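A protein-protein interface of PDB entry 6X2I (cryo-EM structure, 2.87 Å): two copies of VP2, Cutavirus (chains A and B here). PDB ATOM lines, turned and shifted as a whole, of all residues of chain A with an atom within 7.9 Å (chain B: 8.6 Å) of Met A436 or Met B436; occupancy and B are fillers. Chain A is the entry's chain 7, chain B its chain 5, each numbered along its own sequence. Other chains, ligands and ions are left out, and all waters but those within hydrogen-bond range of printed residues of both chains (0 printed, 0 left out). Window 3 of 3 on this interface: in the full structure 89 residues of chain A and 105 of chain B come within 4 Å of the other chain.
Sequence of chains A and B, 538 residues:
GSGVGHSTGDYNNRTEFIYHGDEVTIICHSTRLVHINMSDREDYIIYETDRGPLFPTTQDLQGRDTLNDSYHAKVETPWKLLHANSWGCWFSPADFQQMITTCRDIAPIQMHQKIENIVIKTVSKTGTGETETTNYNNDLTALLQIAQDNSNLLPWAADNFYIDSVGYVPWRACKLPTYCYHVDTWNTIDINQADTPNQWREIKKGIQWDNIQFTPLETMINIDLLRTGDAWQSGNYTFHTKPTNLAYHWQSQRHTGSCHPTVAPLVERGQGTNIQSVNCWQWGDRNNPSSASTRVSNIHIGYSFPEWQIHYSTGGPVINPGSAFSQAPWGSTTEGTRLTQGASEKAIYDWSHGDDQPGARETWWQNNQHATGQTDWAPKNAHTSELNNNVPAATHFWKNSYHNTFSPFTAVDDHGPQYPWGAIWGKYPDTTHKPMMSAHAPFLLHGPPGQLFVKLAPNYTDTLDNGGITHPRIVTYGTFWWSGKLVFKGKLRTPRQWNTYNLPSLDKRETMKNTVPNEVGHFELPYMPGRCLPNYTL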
ATOM      1  N   LYS A 242     -22.858  18.151  22.151  1.00  0.00           N
ATOM      2  CA  LYS A 242     -21.899  18.275  21.072  1.00  0.00           C
ATOM      3  C   LYS A 242     -22.602  18.675  19.784  1.00  0.00           C
ATOM      4  O   LYS A 242     -23.755  18.300  19.565  1.00  0.00           O
ATOM      5  CB  LYS A 242     -21.175  16.949  20.832  1.00  0.00           C
ATOM      6  CG  LYS A 242     -20.295  16.501  21.956  1.00  0.00           C
ATOM      7  CD  LYS A 242     -19.685  15.169  21.606  1.00  0.00           C
ATOM      8  CE  LYS A 242     -20.771  14.123  21.442  1.00  0.00           C
ATOM      9  NZ  LYS A 242     -21.516  13.918  22.710  1.00  0.00           N
ATOM     10  N   ASN A 298      -7.127   1.715   8.183  1.00  0.00           N
ATOM     11  CA  ASN A 298      -7.101   1.890   9.625  1.00  0.00           C
ATOM     12  C   ASN A 298      -8.470   1.681  10.247  1.00  0.00           C
ATOM     13  O   ASN A 298      -8.564   1.266  11.404  1.00  0.00           O
ATOM     14  CB  ASN A 298      -6.583   3.280   9.974  1.00  0.00           C
ATOM     15  CG  ASN A 298      -5.206   3.534   9.437  1.00  0.00           C
ATOM     16  OD1 ASN A 298      -4.929   4.586   8.877  1.00  0.00           O
ATOM     17  ND2 ASN A 298      -4.340   2.557   9.574  1.00  0.00           N
ATOM     18  N   ILE A 299      -9.534   1.954   9.500  1.00  0.00           N
ATOM     19  CA  ILE A 299     -10.894   1.972  10.014  1.00  0.00           C
ATOM     20  C   ILE A 299     -11.786   1.261   9.010  1.00  0.00           C
ATOM     21  O   ILE A 299     -11.358   0.909   7.913  1.00  0.00           O
ATOM     22  CB  ILE A 299     -11.386   3.411  10.284  1.00  0.00           C
ATOM     23  CG1 ILE A 299     -11.412   4.235   9.005  1.00  0.00           C
ATOM     24  CG2 ILE A 299     -10.459   4.112  11.238  1.00  0.00           C
ATOM     25  CD1 ILE A 299     -12.767   4.460   8.446  1.00  0.00           C
ATOM     26  N   PHE A 406     -20.402  -4.764  13.726  1.00  0.00           N
ATOM     27  CA  PHE A 406     -19.937  -3.675  14.569  1.00  0.00           C
ATOM     28  C   PHE A 406     -18.759  -4.142  15.405  1.00  0.00           C
ATOM     29  O   PHE A 406     -18.843  -5.148  16.109  1.00  0.00           O
ATOM     30  CB  PHE A 406     -21.072  -3.174  15.457  1.00  0.00           C
ATOM     31  CG  PHE A 406     -20.664  -2.105  16.421  1.00  0.00           C
ATOM     32  CD1 PHE A 406     -20.439  -0.818  15.992  1.00  0.00           C
ATOM     33  CD2 PHE A 406     -20.538  -2.376  17.762  1.00  0.00           C
ATOM     34  CE1 PHE A 406     -20.068   0.159  16.871  1.00  0.00           C
ATOM     35  CE2 PHE A 406     -20.172  -1.396  18.645  1.00  0.00           C
ATOM     36  CZ  PHE A 406     -19.938  -0.129  18.197  1.00  0.00           C
ATOM     37  N   SER A 407     -17.654  -3.408  15.319  1.00  0.00           N
ATOM     38  CA  SER A 407     -16.373  -3.826  15.862  1.00  0.00           C
ATOM     39  C   SER A 407     -15.665  -2.604  16.426  1.00  0.00           C
ATOM     40  O   SER A 407     -16.225  -1.505  16.383  1.00  0.00           O
ATOM     41  CB  SER A 407     -15.541  -4.489  14.769  1.00  0.00           C
ATOM     42  OG  SER A 407     -15.180  -3.550  13.777  1.00  0.00           O
ATOM     43  N   PRO A 408     -14.451  -2.732  16.974  1.00  0.00           N
ATOM     44  CA  PRO A 408     -13.733  -1.527  17.406  1.00  0.00           C
ATOM     45  C   PRO A 408     -13.307  -0.645  16.257  1.00  0.00           C
ATOM     46  O   PRO A 408     -12.946   0.513  16.484  1.00  0.00           O
ATOM     47  CB  PRO A 408     -12.517  -2.088  18.146  1.00  0.00           C
ATOM     48  CG  PRO A 408     -12.910  -3.426  18.541  1.00  0.00           C
ATOM     49  CD  PRO A 408     -13.766  -3.941  17.452  1.00  0.00           C
ATOM     50  N   PHE A 409     -13.326  -1.161  15.038  1.00  0.00           N
ATOM     51  CA  PHE A 409     -12.815  -0.458  13.875  1.00  0.00           C
ATOM     52  C   PHE A 409     -13.872   0.341  13.134  1.00  0.00           C
ATOM     53  O   PHE A 409     -13.518   1.136  12.264  1.00  0.00           O
ATOM     54  CB  PHE A 409     -12.195  -1.470  12.916  1.00  0.00           C
ATOM     55  CG  PHE A 409     -11.078  -2.259  13.516  1.00  0.00           C
ATOM     56  CD1 PHE A 409     -10.304  -1.734  14.519  1.00  0.00           C
ATOM     57  CD2 PHE A 409     -10.848  -3.551  13.117  1.00  0.00           C
ATOM     58  CE1 PHE A 409      -9.298  -2.461  15.073  1.00  0.00           C
ATOM     59  CE2 PHE A 409      -9.845  -4.281  13.675  1.00  0.00           C
ATOM     60  CZ  PHE A 409      -9.071  -3.736  14.654  1.00  0.00           C
ATOM     61  N   THR A 410     -15.150   0.173  13.454  1.00  0.00           N
ATOM     62  CA  THR A 410     -16.199   0.724  12.611  1.00  0.00           C
ATOM     63  C   THR A 410     -16.420   2.198  12.905  1.00  0.00           C
ATOM     64  O   THR A 410     -16.604   2.594  14.057  1.00  0.00           O
ATOM     65  CB  THR A 410     -17.510  -0.037  12.784  1.00  0.00           C
ATOM     66  OG1 THR A 410     -17.915   0.007  14.150  1.00  0.00           O
ATOM     67  CG2 THR A 410     -17.347  -1.476  12.355  1.00  0.00           C
ATOM     68  N   ALA A 411     -16.391   3.002  11.851  1.00  0.00           N
ATOM     69  CA  ALA A 411     -16.820   4.386  11.888  1.00  0.00           C
ATOM     70  C   ALA A 411     -18.187   4.465  11.236  1.00  0.00           C
ATOM     71  O   ALA A 411     -18.370   3.981  10.119  1.00  0.00           O
ATOM     72  CB  ALA A 411     -15.827   5.284  11.157  1.00  0.00           C
ATOM     73  N   VAL A 412     -19.147   5.056  11.934  1.00  0.00           N
ATOM     74  CA  VAL A 412     -20.533   5.047  11.499  1.00  0.00           C
ATOM     75  C   VAL A 412     -21.121   6.416  11.810  1.00  0.00           C
ATOM     76  O   VAL A 412     -20.476   7.262  12.427  1.00  0.00           O
ATOM     77  CB  VAL A 412     -21.320   3.905  12.184  1.00  0.00           C
ATOM     78  CG1 VAL A 412     -21.511   4.188  13.653  1.00  0.00           C
ATOM     79  CG2 VAL A 412     -22.613   3.593  11.482  1.00  0.00           C
ATOM     80  N   TYR A 428     -30.709  10.491  27.802  1.00  0.00           N
ATOM     81  CA  TYR A 428     -29.976   9.277  28.105  1.00  0.00           C
ATOM     82  C   TYR A 428     -30.714   8.459  29.158  1.00  0.00           C
ATOM     83  O   TYR A 428     -31.339   9.012  30.061  1.00  0.00           O
ATOM     84  CB  TYR A 428     -28.577   9.565  28.631  1.00  0.00           C
ATOM     85  CG  TYR A 428     -27.553  10.020  27.633  1.00  0.00           C
ATOM     86  CD1 TYR A 428     -26.946   9.116  26.786  1.00  0.00           C
ATOM     87  CD2 TYR A 428     -27.114  11.324  27.613  1.00  0.00           C
ATOM     88  CE1 TYR A 428     -25.984   9.518  25.896  1.00  0.00           C
ATOM     89  CE2 TYR A 428     -26.151  11.733  26.731  1.00  0.00           C
ATOM     90  CZ  TYR A 428     -25.589  10.828  25.876  1.00  0.00           C
ATOM     91  OH  TYR A 428     -24.625  11.243  24.993  1.00  0.00           O
ATOM     92  N   HIS A 433     -23.660   1.421  31.082  1.00  0.00           N
ATOM     93  CA  HIS A 433     -23.178   1.687  29.737  1.00  0.00           C
ATOM     94  C   HIS A 433     -24.181   2.580  29.022  1.00  0.00           C
ATOM     95  O   HIS A 433     -25.285   2.142  28.695  1.00  0.00           O
ATOM     96  CB  HIS A 433     -22.960   0.388  28.973  1.00  0.00           C
ATOM     97  CG  HIS A 433     -22.477   0.597  27.576  1.00  0.00           C
ATOM     98  ND1 HIS A 433     -21.295   1.241  27.288  1.00  0.00           N
ATOM     99  CD2 HIS A 433     -23.023   0.261  26.385  1.00  0.00           C
ATOM    100  CE1 HIS A 433     -21.135   1.293  25.981  1.00  0.00           C
ATOM    101  NE2 HIS A 433     -22.167   0.704  25.408  1.00  0.00           N
ATOM    102  N   LYS A 434     -23.795   3.823  28.776  1.00  0.00           N
ATOM    103  CA  LYS A 434     -24.632   4.701  27.982  1.00  0.00           C
ATOM    104  C   LYS A 434     -24.438   4.415  26.499  1.00  0.00           C
ATOM    105  O   LYS A 434     -23.350   4.029  26.074  1.00  0.00           O
ATOM    106  CB  LYS A 434     -24.302   6.162  28.255  1.00  0.00           C
ATOM    107  CG  LYS A 434     -25.106   6.812  29.356  1.00  0.00           C
ATOM    108  CD  LYS A 434     -24.718   6.287  30.709  1.00  0.00           C
ATOM    109  CE  LYS A 434     -25.511   6.960  31.792  1.00  0.00           C
ATOM    110  NZ  LYS A 434     -25.101   6.471  33.124  1.00  0.00           N
ATOM    111  N   PRO A 435     -25.477   4.605  25.692  1.00  0.00           N
ATOM    112  CA  PRO A 435     -25.336   4.399  24.253  1.00  0.00           C
ATOM    113  C   PRO A 435     -24.316   5.345  23.649  1.00  0.00           C
ATOM    114  O   PRO A 435     -24.099   6.456  24.132  1.00  0.00           O
ATOM    115  CB  PRO A 435     -26.741   4.686  23.725  1.00  0.00           C
ATOM    116  CG  PRO A 435     -27.608   4.394  24.858  1.00  0.00           C
ATOM    117  CD  PRO A 435     -26.872   4.859  26.063  1.00  0.00           C
ATOM    118  N   MET A 436     -23.681   4.889  22.576  1.00  0.00           N
ATOM    119  CA  MET A 436     -22.641   5.693  21.955  1.00  0.00           C
ATOM    120  C   MET A 436     -23.221   6.777  21.065  1.00  0.00           C
ATOM    121  O   MET A 436     -22.598   7.825  20.883  1.00  0.00           O
ATOM    122  CB  MET A 436     -21.719   4.800  21.141  1.00  0.00           C
ATOM    123  CG  MET A 436     -21.078   3.727  21.958  1.00  0.00           C
ATOM    124  SD  MET A 436     -20.218   2.559  20.917  1.00  0.00           S
ATOM    125  CE  MET A 436     -19.868   1.322  22.131  1.00  0.00           C
ATOM    126  N   MET A 437     -24.393   6.539  20.493  1.00  0.00           N
ATOM    127  CA  MET A 437     -24.981   7.491  19.569  1.00  0.00           C
ATOM    128  C   MET A 437     -26.471   7.218  19.494  1.00  0.00           C
ATOM    129  O   MET A 437     -26.946   6.167  19.917  1.00  0.00           O
ATOM    130  CB  MET A 437     -24.303   7.399  18.205  1.00  0.00           C
ATOM    131  CG  MET A 437     -24.501   6.079  17.537  1.00  0.00           C
ATOM    132  SD  MET A 437     -23.518   5.904  16.050  1.00  0.00           S
ATOM    133  CE  MET A 437     -24.396   6.964  14.950  1.00  0.00           C
ATOM    134  N   SER A 438     -27.201   8.185  18.965  1.00  0.00           N
ATOM    135  CA  SER A 438     -28.652   8.162  18.981  1.00  0.00           C
ATOM    136  C   SER A 438     -29.210   7.630  17.672  1.00  0.00           C
ATOM    137  O   SER A 438     -28.646   7.846  16.600  1.00  0.00           O
ATOM    138  CB  SER A 438     -29.203   9.556  19.244  1.00  0.00           C
ATOM    139  OG  SER A 438     -30.611   9.548  19.206  1.00  0.00           O
ATOM    140  N   ALA A 439     -30.319   6.906  17.774  1.00  0.00           N
ATOM    141  CA  ALA A 439     -31.012   6.392  16.606  1.00  0.00           C
ATOM    142  C   ALA A 439     -32.042   7.354  16.040  1.00  0.00           C
ATOM    143  O   ALA A 439     -32.530   7.121  14.937  1.00  0.00           O
ATOM    144  CB  ALA A 439     -31.696   5.069  16.936  1.00  0.00           C
ATOM    145  N   LEU A 444     -28.518  13.784  22.553  1.00  0.00           N
ATOM    146  CA  LEU A 444     -28.918  13.096  23.769  1.00  0.00           C
ATOM    147  C   LEU A 444     -28.401  13.879  24.960  1.00  0.00           C
ATOM    148  O   LEU A 444     -27.245  14.308  24.971  1.00  0.00           O
ATOM    149  CB  LEU A 444     -28.392  11.666  23.811  1.00  0.00           C
ATOM    150  CG  LEU A 444     -28.941  10.696  22.775  1.00  0.00           C
ATOM    151  CD1 LEU A 444     -28.275   9.357  22.926  1.00  0.00           C
ATOM    152  CD2 LEU A 444     -30.425  10.564  22.931  1.00  0.00           C
ATOM    153  N   LYS B 242      -1.987   9.206  22.092  1.00  0.00           N
ATOM    154  CA  LYS B 242      -1.689   8.359  23.229  1.00  0.00           C
ATOM    155  C   LYS B 242      -0.538   7.421  22.904  1.00  0.00           C
ATOM    156  O   LYS B 242      -0.380   7.011  21.752  1.00  0.00           O
ATOM    157  CB  LYS B 242      -2.904   7.513  23.611  1.00  0.00           C
ATOM    158  CG  LYS B 242      -4.076   8.292  24.123  1.00  0.00           C
ATOM    159  CD  LYS B 242      -5.210   7.343  24.416  1.00  0.00           C
ATOM    160  CE  LYS B 242      -5.654   6.649  23.142  1.00  0.00           C
ATOM    161  NZ  LYS B 242      -6.174   7.625  22.151  1.00  0.00           N
ATOM    162  N   PHE B 406     -17.814  -9.425  19.947  1.00  0.00           N
ATOM    163  CA  PHE B 406     -17.451  -8.137  20.519  1.00  0.00           C
ATOM    164  C   PHE B 406     -18.599  -7.610  21.361  1.00  0.00           C
ATOM    165  O   PHE B 406     -19.731  -7.502  20.888  1.00  0.00           O
ATOM    166  CB  PHE B 406     -17.087  -7.152  19.412  1.00  0.00           C
ATOM    167  CG  PHE B 406     -16.780  -5.772  19.904  1.00  0.00           C
ATOM    168  CD1 PHE B 406     -15.588  -5.498  20.533  1.00  0.00           C
ATOM    169  CD2 PHE B 406     -17.667  -4.740  19.708  1.00  0.00           C
ATOM    170  CE1 PHE B 406     -15.306  -4.238  20.981  1.00  0.00           C
ATOM    171  CE2 PHE B 406     -17.381  -3.476  20.149  1.00  0.00           C
ATOM    172  CZ  PHE B 406     -16.201  -3.228  20.787  1.00  0.00           C
ATOM    173  N   SER B 407     -18.304  -7.288  22.615  1.00  0.00           N
ATOM    174  CA  SER B 407     -19.310  -6.987  23.621  1.00  0.00           C
ATOM    175  C   SER B 407     -18.786  -5.870  24.510  1.00  0.00           C
ATOM    176  O   SER B 407     -17.678  -5.377  24.275  1.00  0.00           O
ATOM    177  CB  SER B 407     -19.615  -8.240  24.436  1.00  0.00           C
ATOM    178  OG  SER B 407     -18.495  -8.622  25.204  1.00  0.00           O
ATOM    179  N   PRO B 408     -19.532  -5.422  25.526  1.00  0.00           N
ATOM    180  CA  PRO B 408     -18.964  -4.427  26.443  1.00  0.00           C
ATOM    181  C   PRO B 408     -17.837  -4.972  27.288  1.00  0.00           C
ATOM    182  O   PRO B 408     -17.099  -4.190  27.893  1.00  0.00           O
ATOM    183  CB  PRO B 408     -20.158  -4.029  27.313  1.00  0.00           C
ATOM    184  CG  PRO B 408     -21.322  -4.364  26.519  1.00  0.00           C
ATOM    185  CD  PRO B 408     -20.970  -5.589  25.771  1.00  0.00           C
ATOM    186  N   THR B 410     -15.276  -7.051  26.268  1.00  0.00           N
ATOM    187  CA  THR B 410     -14.095  -7.537  25.572  1.00  0.00           C
ATOM    188  C   THR B 410     -12.942  -6.557  25.695  1.00  0.00           C
ATOM    189  O   THR B 410     -13.090  -5.365  25.415  1.00  0.00           O
ATOM    190  CB  THR B 410     -14.387  -7.805  24.099  1.00  0.00           C
ATOM    191  OG1 THR B 410     -14.856  -6.611  23.476  1.00  0.00           O
ATOM    192  CG2 THR B 410     -15.431  -8.887  23.954  1.00  0.00           C
ATOM    193  N   VAL B 412      -9.260  -6.057  24.037  1.00  0.00           N
ATOM    194  CA  VAL B 412      -8.626  -6.479  22.801  1.00  0.00           C
ATOM    195  C   VAL B 412      -7.451  -5.545  22.547  1.00  0.00           C
ATOM    196  O   VAL B 412      -7.243  -4.571  23.267  1.00  0.00           O
ATOM    197  CB  VAL B 412      -9.638  -6.476  21.631  1.00  0.00           C
ATOM    198  CG1 VAL B 412     -10.023  -5.067  21.255  1.00  0.00           C
ATOM    199  CG2 VAL B 412      -9.158  -7.279  20.452  1.00  0.00           C
ATOM    200  N   ASP B 414      -4.332  -4.136  19.430  1.00  0.00           N
ATOM    201  CA  ASP B 414      -4.156  -3.867  18.010  1.00  0.00           C
ATOM    202  C   ASP B 414      -2.850  -4.459  17.483  1.00  0.00           C
ATOM    203  O   ASP B 414      -2.137  -5.182  18.180  1.00  0.00           O
ATOM    204  CB  ASP B 414      -4.219  -2.367  17.750  1.00  0.00           C
ATOM    205  CG  ASP B 414      -3.164  -1.612  18.494  1.00  0.00           C
ATOM    206  OD1 ASP B 414      -2.459  -2.245  19.303  1.00  0.00           O
ATOM    207  OD2 ASP B 414      -3.029  -0.392  18.272  1.00  0.00           O
ATOM    208  N   TYR B 428      -8.443  10.066  11.611  1.00  0.00           N
ATOM    209  CA  TYR B 428      -9.821   9.746  11.932  1.00  0.00           C
ATOM    210  C   TYR B 428     -10.751  10.231  10.827  1.00  0.00           C
ATOM    211  O   TYR B 428     -10.514  11.272  10.215  1.00  0.00           O
ATOM    212  CB  TYR B 428     -10.272  10.387  13.238  1.00  0.00           C
ATOM    213  CG  TYR B 428      -9.759   9.779  14.509  1.00  0.00           C
ATOM    214  CD1 TYR B 428     -10.306   8.612  15.003  1.00  0.00           C
ATOM    215  CD2 TYR B 428      -8.811  10.422  15.271  1.00  0.00           C
ATOM    216  CE1 TYR B 428      -9.869   8.067  16.182  1.00  0.00           C
ATOM    217  CE2 TYR B 428      -8.371   9.889  16.453  1.00  0.00           C
ATOM    218  CZ  TYR B 428      -8.901   8.714  16.904  1.00  0.00           C
ATOM    219  OH  TYR B 428      -8.455   8.183  18.087  1.00  0.00           O
ATOM    220  N   PRO B 429     -11.824   9.503  10.562  1.00  0.00           N
ATOM    221  CA  PRO B 429     -12.932  10.079   9.807  1.00  0.00           C
ATOM    222  C   PRO B 429     -13.748  10.974  10.715  1.00  0.00           C
ATOM    223  O   PRO B 429     -13.778  10.792  11.931  1.00  0.00           O
ATOM    224  CB  PRO B 429     -13.736   8.848   9.386  1.00  0.00           C
ATOM    225  CG  PRO B 429     -13.499   7.898  10.488  1.00  0.00           C
ATOM    226  CD  PRO B 429     -12.098   8.113  10.956  1.00  0.00           C
ATOM    227  N   THR B 432     -20.208  10.666  13.545  1.00  0.00           N
ATOM    228  CA  THR B 432     -20.706  10.790  14.906  1.00  0.00           C
ATOM    229  C   THR B 432     -20.051   9.778  15.829  1.00  0.00           C
ATOM    230  O   THR B 432     -19.836  10.067  17.010  1.00  0.00           O
ATOM    231  CB  THR B 432     -22.219  10.648  14.929  1.00  0.00           C
ATOM    232  OG1 THR B 432     -22.586   9.434  14.281  1.00  0.00           O
ATOM    233  CG2 THR B 432     -22.849  11.801  14.212  1.00  0.00           C
ATOM    234  N   HIS B 433     -19.708   8.607  15.314  1.00  0.00           N
ATOM    235  CA  HIS B 433     -19.017   7.586  16.087  1.00  0.00           C
ATOM    236  C   HIS B 433     -17.629   7.381  15.501  1.00  0.00           C
ATOM    237  O   HIS B 433     -17.487   6.847  14.399  1.00  0.00           O
ATOM    238  CB  HIS B 433     -19.806   6.284  16.092  1.00  0.00           C
ATOM    239  CG  HIS B 433     -19.141   5.190  16.859  1.00  0.00           C
ATOM    240  ND1 HIS B 433     -18.850   5.296  18.200  1.00  0.00           N
ATOM    241  CD2 HIS B 433     -18.692   3.975  16.470  1.00  0.00           C
ATOM    242  CE1 HIS B 433     -18.251   4.193  18.606  1.00  0.00           C
ATOM    243  NE2 HIS B 433     -18.145   3.374  17.576  1.00  0.00           N
ATOM    244  N   LYS B 434     -16.610   7.796  16.237  1.00  0.00           N
ATOM    245  CA  LYS B 434     -15.249   7.521  15.820  1.00  0.00           C
ATOM    246  C   LYS B 434     -14.859   6.098  16.199  1.00  0.00           C
ATOM    247  O   LYS B 434     -15.329   5.570  17.205  1.00  0.00           O
ATOM    248  CB  LYS B 434     -14.272   8.494  16.466  1.00  0.00           C
ATOM    249  CG  LYS B 434     -13.989   9.747  15.674  1.00  0.00           C
ATOM    250  CD  LYS B 434     -15.175  10.672  15.657  1.00  0.00           C
ATOM    251  CE  LYS B 434     -14.868  11.922  14.884  1.00  0.00           C
ATOM    252  NZ  LYS B 434     -16.019  12.846  14.901  1.00  0.00           N
ATOM    253  N   PRO B 435     -13.997   5.463  15.412  1.00  0.00           N
ATOM    254  CA  PRO B 435     -13.546   4.116  15.752  1.00  0.00           C
ATOM    255  C   PRO B 435     -12.808   4.093  17.079  1.00  0.00           C
ATOM    256  O   PRO B 435     -12.181   5.071  17.487  1.00  0.00           O
ATOM    257  CB  PRO B 435     -12.617   3.761  14.593  1.00  0.00           C
ATOM    258  CG  PRO B 435     -13.108   4.572  13.489  1.00  0.00           C
ATOM    259  CD  PRO B 435     -13.516   5.871  14.088  1.00  0.00           C
ATOM    260  N   MET B 436     -12.890   2.955  17.756  1.00  0.00           N
ATOM    261  CA  MET B 436     -12.267   2.847  19.066  1.00  0.00           C
ATOM    262  C   MET B 436     -10.775   2.597  18.962  1.00  0.00           C
ATOM    263  O   MET B 436     -10.022   2.979  19.861  1.00  0.00           O
ATOM    264  CB  MET B 436     -12.922   1.724  19.853  1.00  0.00           C
ATOM    265  CG  MET B 436     -14.393   1.917  20.031  1.00  0.00           C
ATOM    266  SD  MET B 436     -15.149   0.459  20.729  1.00  0.00           S
ATOM    267  CE  MET B 436     -16.847   0.908  20.516  1.00  0.00           C
ATOM    268  N   MET B 437     -10.333   1.948  17.894  1.00  0.00           N
ATOM    269  CA  MET B 437      -8.930   1.603  17.756  1.00  0.00           C
ATOM    270  C   MET B 437      -8.648   1.359  16.285  1.00  0.00           C
ATOM    271  O   MET B 437      -9.562   1.190  15.482  1.00  0.00           O
ATOM    272  CB  MET B 437      -8.590   0.395  18.622  1.00  0.00           C
ATOM    273  CG  MET B 437      -9.309  -0.847  18.211  1.00  0.00           C
ATOM    274  SD  MET B 437      -9.077  -2.194  19.368  1.00  0.00           S
ATOM    275  CE  MET B 437      -7.411  -2.646  19.014  1.00  0.00           C
ATOM    276  N   SER B 438      -7.371   1.361  15.944  1.00  0.00           N
ATOM    277  CA  SER B 438      -6.935   1.320  14.560  1.00  0.00           C
ATOM    278  C   SER B 438      -6.591  -0.097  14.130  1.00  0.00           C
ATOM    279  O   SER B 438      -6.094  -0.902  14.917  1.00  0.00           O
ATOM    280  CB  SER B 438      -5.730   2.224  14.355  1.00  0.00           C
ATOM    281  OG  SER B 438      -5.270   2.147  13.026  1.00  0.00           O
ATOM    282  N   ALA B 439      -6.883  -0.401  12.871  1.00  0.00           N
ATOM    283  CA  ALA B 439      -6.547  -1.690  12.292  1.00  0.00           C
ATOM    284  C   ALA B 439      -5.162  -1.731  11.673  1.00  0.00           C
ATOM    285  O   ALA B 439      -4.688  -2.820  11.351  1.00  0.00           O
ATOM    286  CB  ALA B 439      -7.577  -2.081  11.237  1.00  0.00           C
ATOM    287  N   LEU B 444      -3.984   7.217  15.509  1.00  0.00           N
ATOM    288  CA  LEU B 444      -4.990   7.917  14.728  1.00  0.00           C
ATOM    289  C   LEU B 444      -5.059   9.354  15.207  1.00  0.00           C
ATOM    290  O   LEU B 444      -5.077   9.611  16.412  1.00  0.00           O
ATOM    291  CB  LEU B 444      -6.359   7.258  14.844  1.00  0.00           C
ATOM    292  CG  LEU B 444      -6.506   5.861  14.258  1.00  0.00           C
ATOM    293  CD1 LEU B 444      -7.895   5.345  14.511  1.00  0.00           C
ATOM    294  CD2 LEU B 444      -6.216   5.887  12.790  1.00  0.00           C
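N of His B433 sits at hydrogen-bond distance from O of Val A412 (3.3 Å).
The backbone NH (N) of Met B436 is in hydrogen-bond range of the backbone carbonyl oxygen (O) of Pro A408, at 2.8 Å.
O of Pro A408 is in hydrogen-bond range of N of Met B437, at 3.3 Å.
The backbone NH (N) of Ala B439 is in hydrogen-bond range of the backbone carbonyl oxygen (O) of Asn A298, 2.8 Å away.
OG of Ser A407 lies close to N of Phe A409 (3.3 Å).
The backbone carbonyl oxygen of Ser A407 sits at hydrogen-bond distance from the side-chain hydroxyl of Thr A410.
Among the printed residues, pairs that only touch across the chains: Asn A298 with Ser B438 (3.5 Å), Asn A298 with Leu B444 (3.9 Å), Ile A299 with Pro B435 (3.5 Å), Phe A406 with Phe B406 (3.8 Å), Phe A406 with His B433 (3.8 Å), Pro A408 with Phe B406 (3.5 Å), Pro A408 with Pro B435 (3.6 Å), Phe A409 with Pro B435 (3.6 Å), Phe A409 with Met B437 (3.2 Å), Phe A409 with Ser B438 (3.6 Å), Phe A409 with Ala B439 (3.9 Å), Thr A410 with His B433 (3.5 Å), Thr A410 with Pro B435 (3.8 Å), Ala A411 with Pro B429 (3.6 Å), Ala A411 with His B433 (3.6 Å), Ala A411 with Pro B435 (3.7 Å), Val A412 with Thr B432 (3.6 Å), Met A436 with His B433 (3.4 Å), Met A436 with Met B436 (3.5 Å), Met A437 with Thr B432 (3.1 Å) and Met A437 with His B433 (3.7 Å).
Met A436 touches just these residues of chain B: His B433 (3.4 Å) and Met B436 (3.5 Å).
Of the printed residues of chain A, Met B436 touches Pro A408 and Met A436.
Printed residues of chain A within 4 Å of Pro B429: Ala A411 (3.6 Å).
Of the printed residues of chain A, Ser B438 touches Asn A298 and Phe A409.
Printed residues of chain A within 4 Å of Leu B444: Asn A298.
The nearest residue of chain B that does not touch Met A436 is Thr B432 (5.3 Å).
Printed residues of chain A that touch a printed residue of chain B: Asn A298, Ile A299, Phe A406, Pro A408, Phe A409, Thr A410, Ala A411, Val A412, Met A436 and Met A437.
Among the printed residues, 25 pairs touch across the chains.
Among the printed residues, no Asp or Glu carboxylate lies within 4 Å of a Lys or Arg side-chain nitrogen of the other chain.
Phe B406 touches its own counterpart, Phe A406.
Phe A406 touches His B433, but with the chains exchanged His A433 does not touch Phe B406 (8.2 Å).
Pro A408 touches Met B436, but with the chains exchanged Met A436 does not touch Pro B408 (7.2 Å).
Met A437 touches His B433, but with the chains exchanged His A433 does not touch Met B437 (13.5 Å).
Of the 25 pairs that touch across the chains among the printed residues, 2 have their exchanged pair printed and touching as well.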
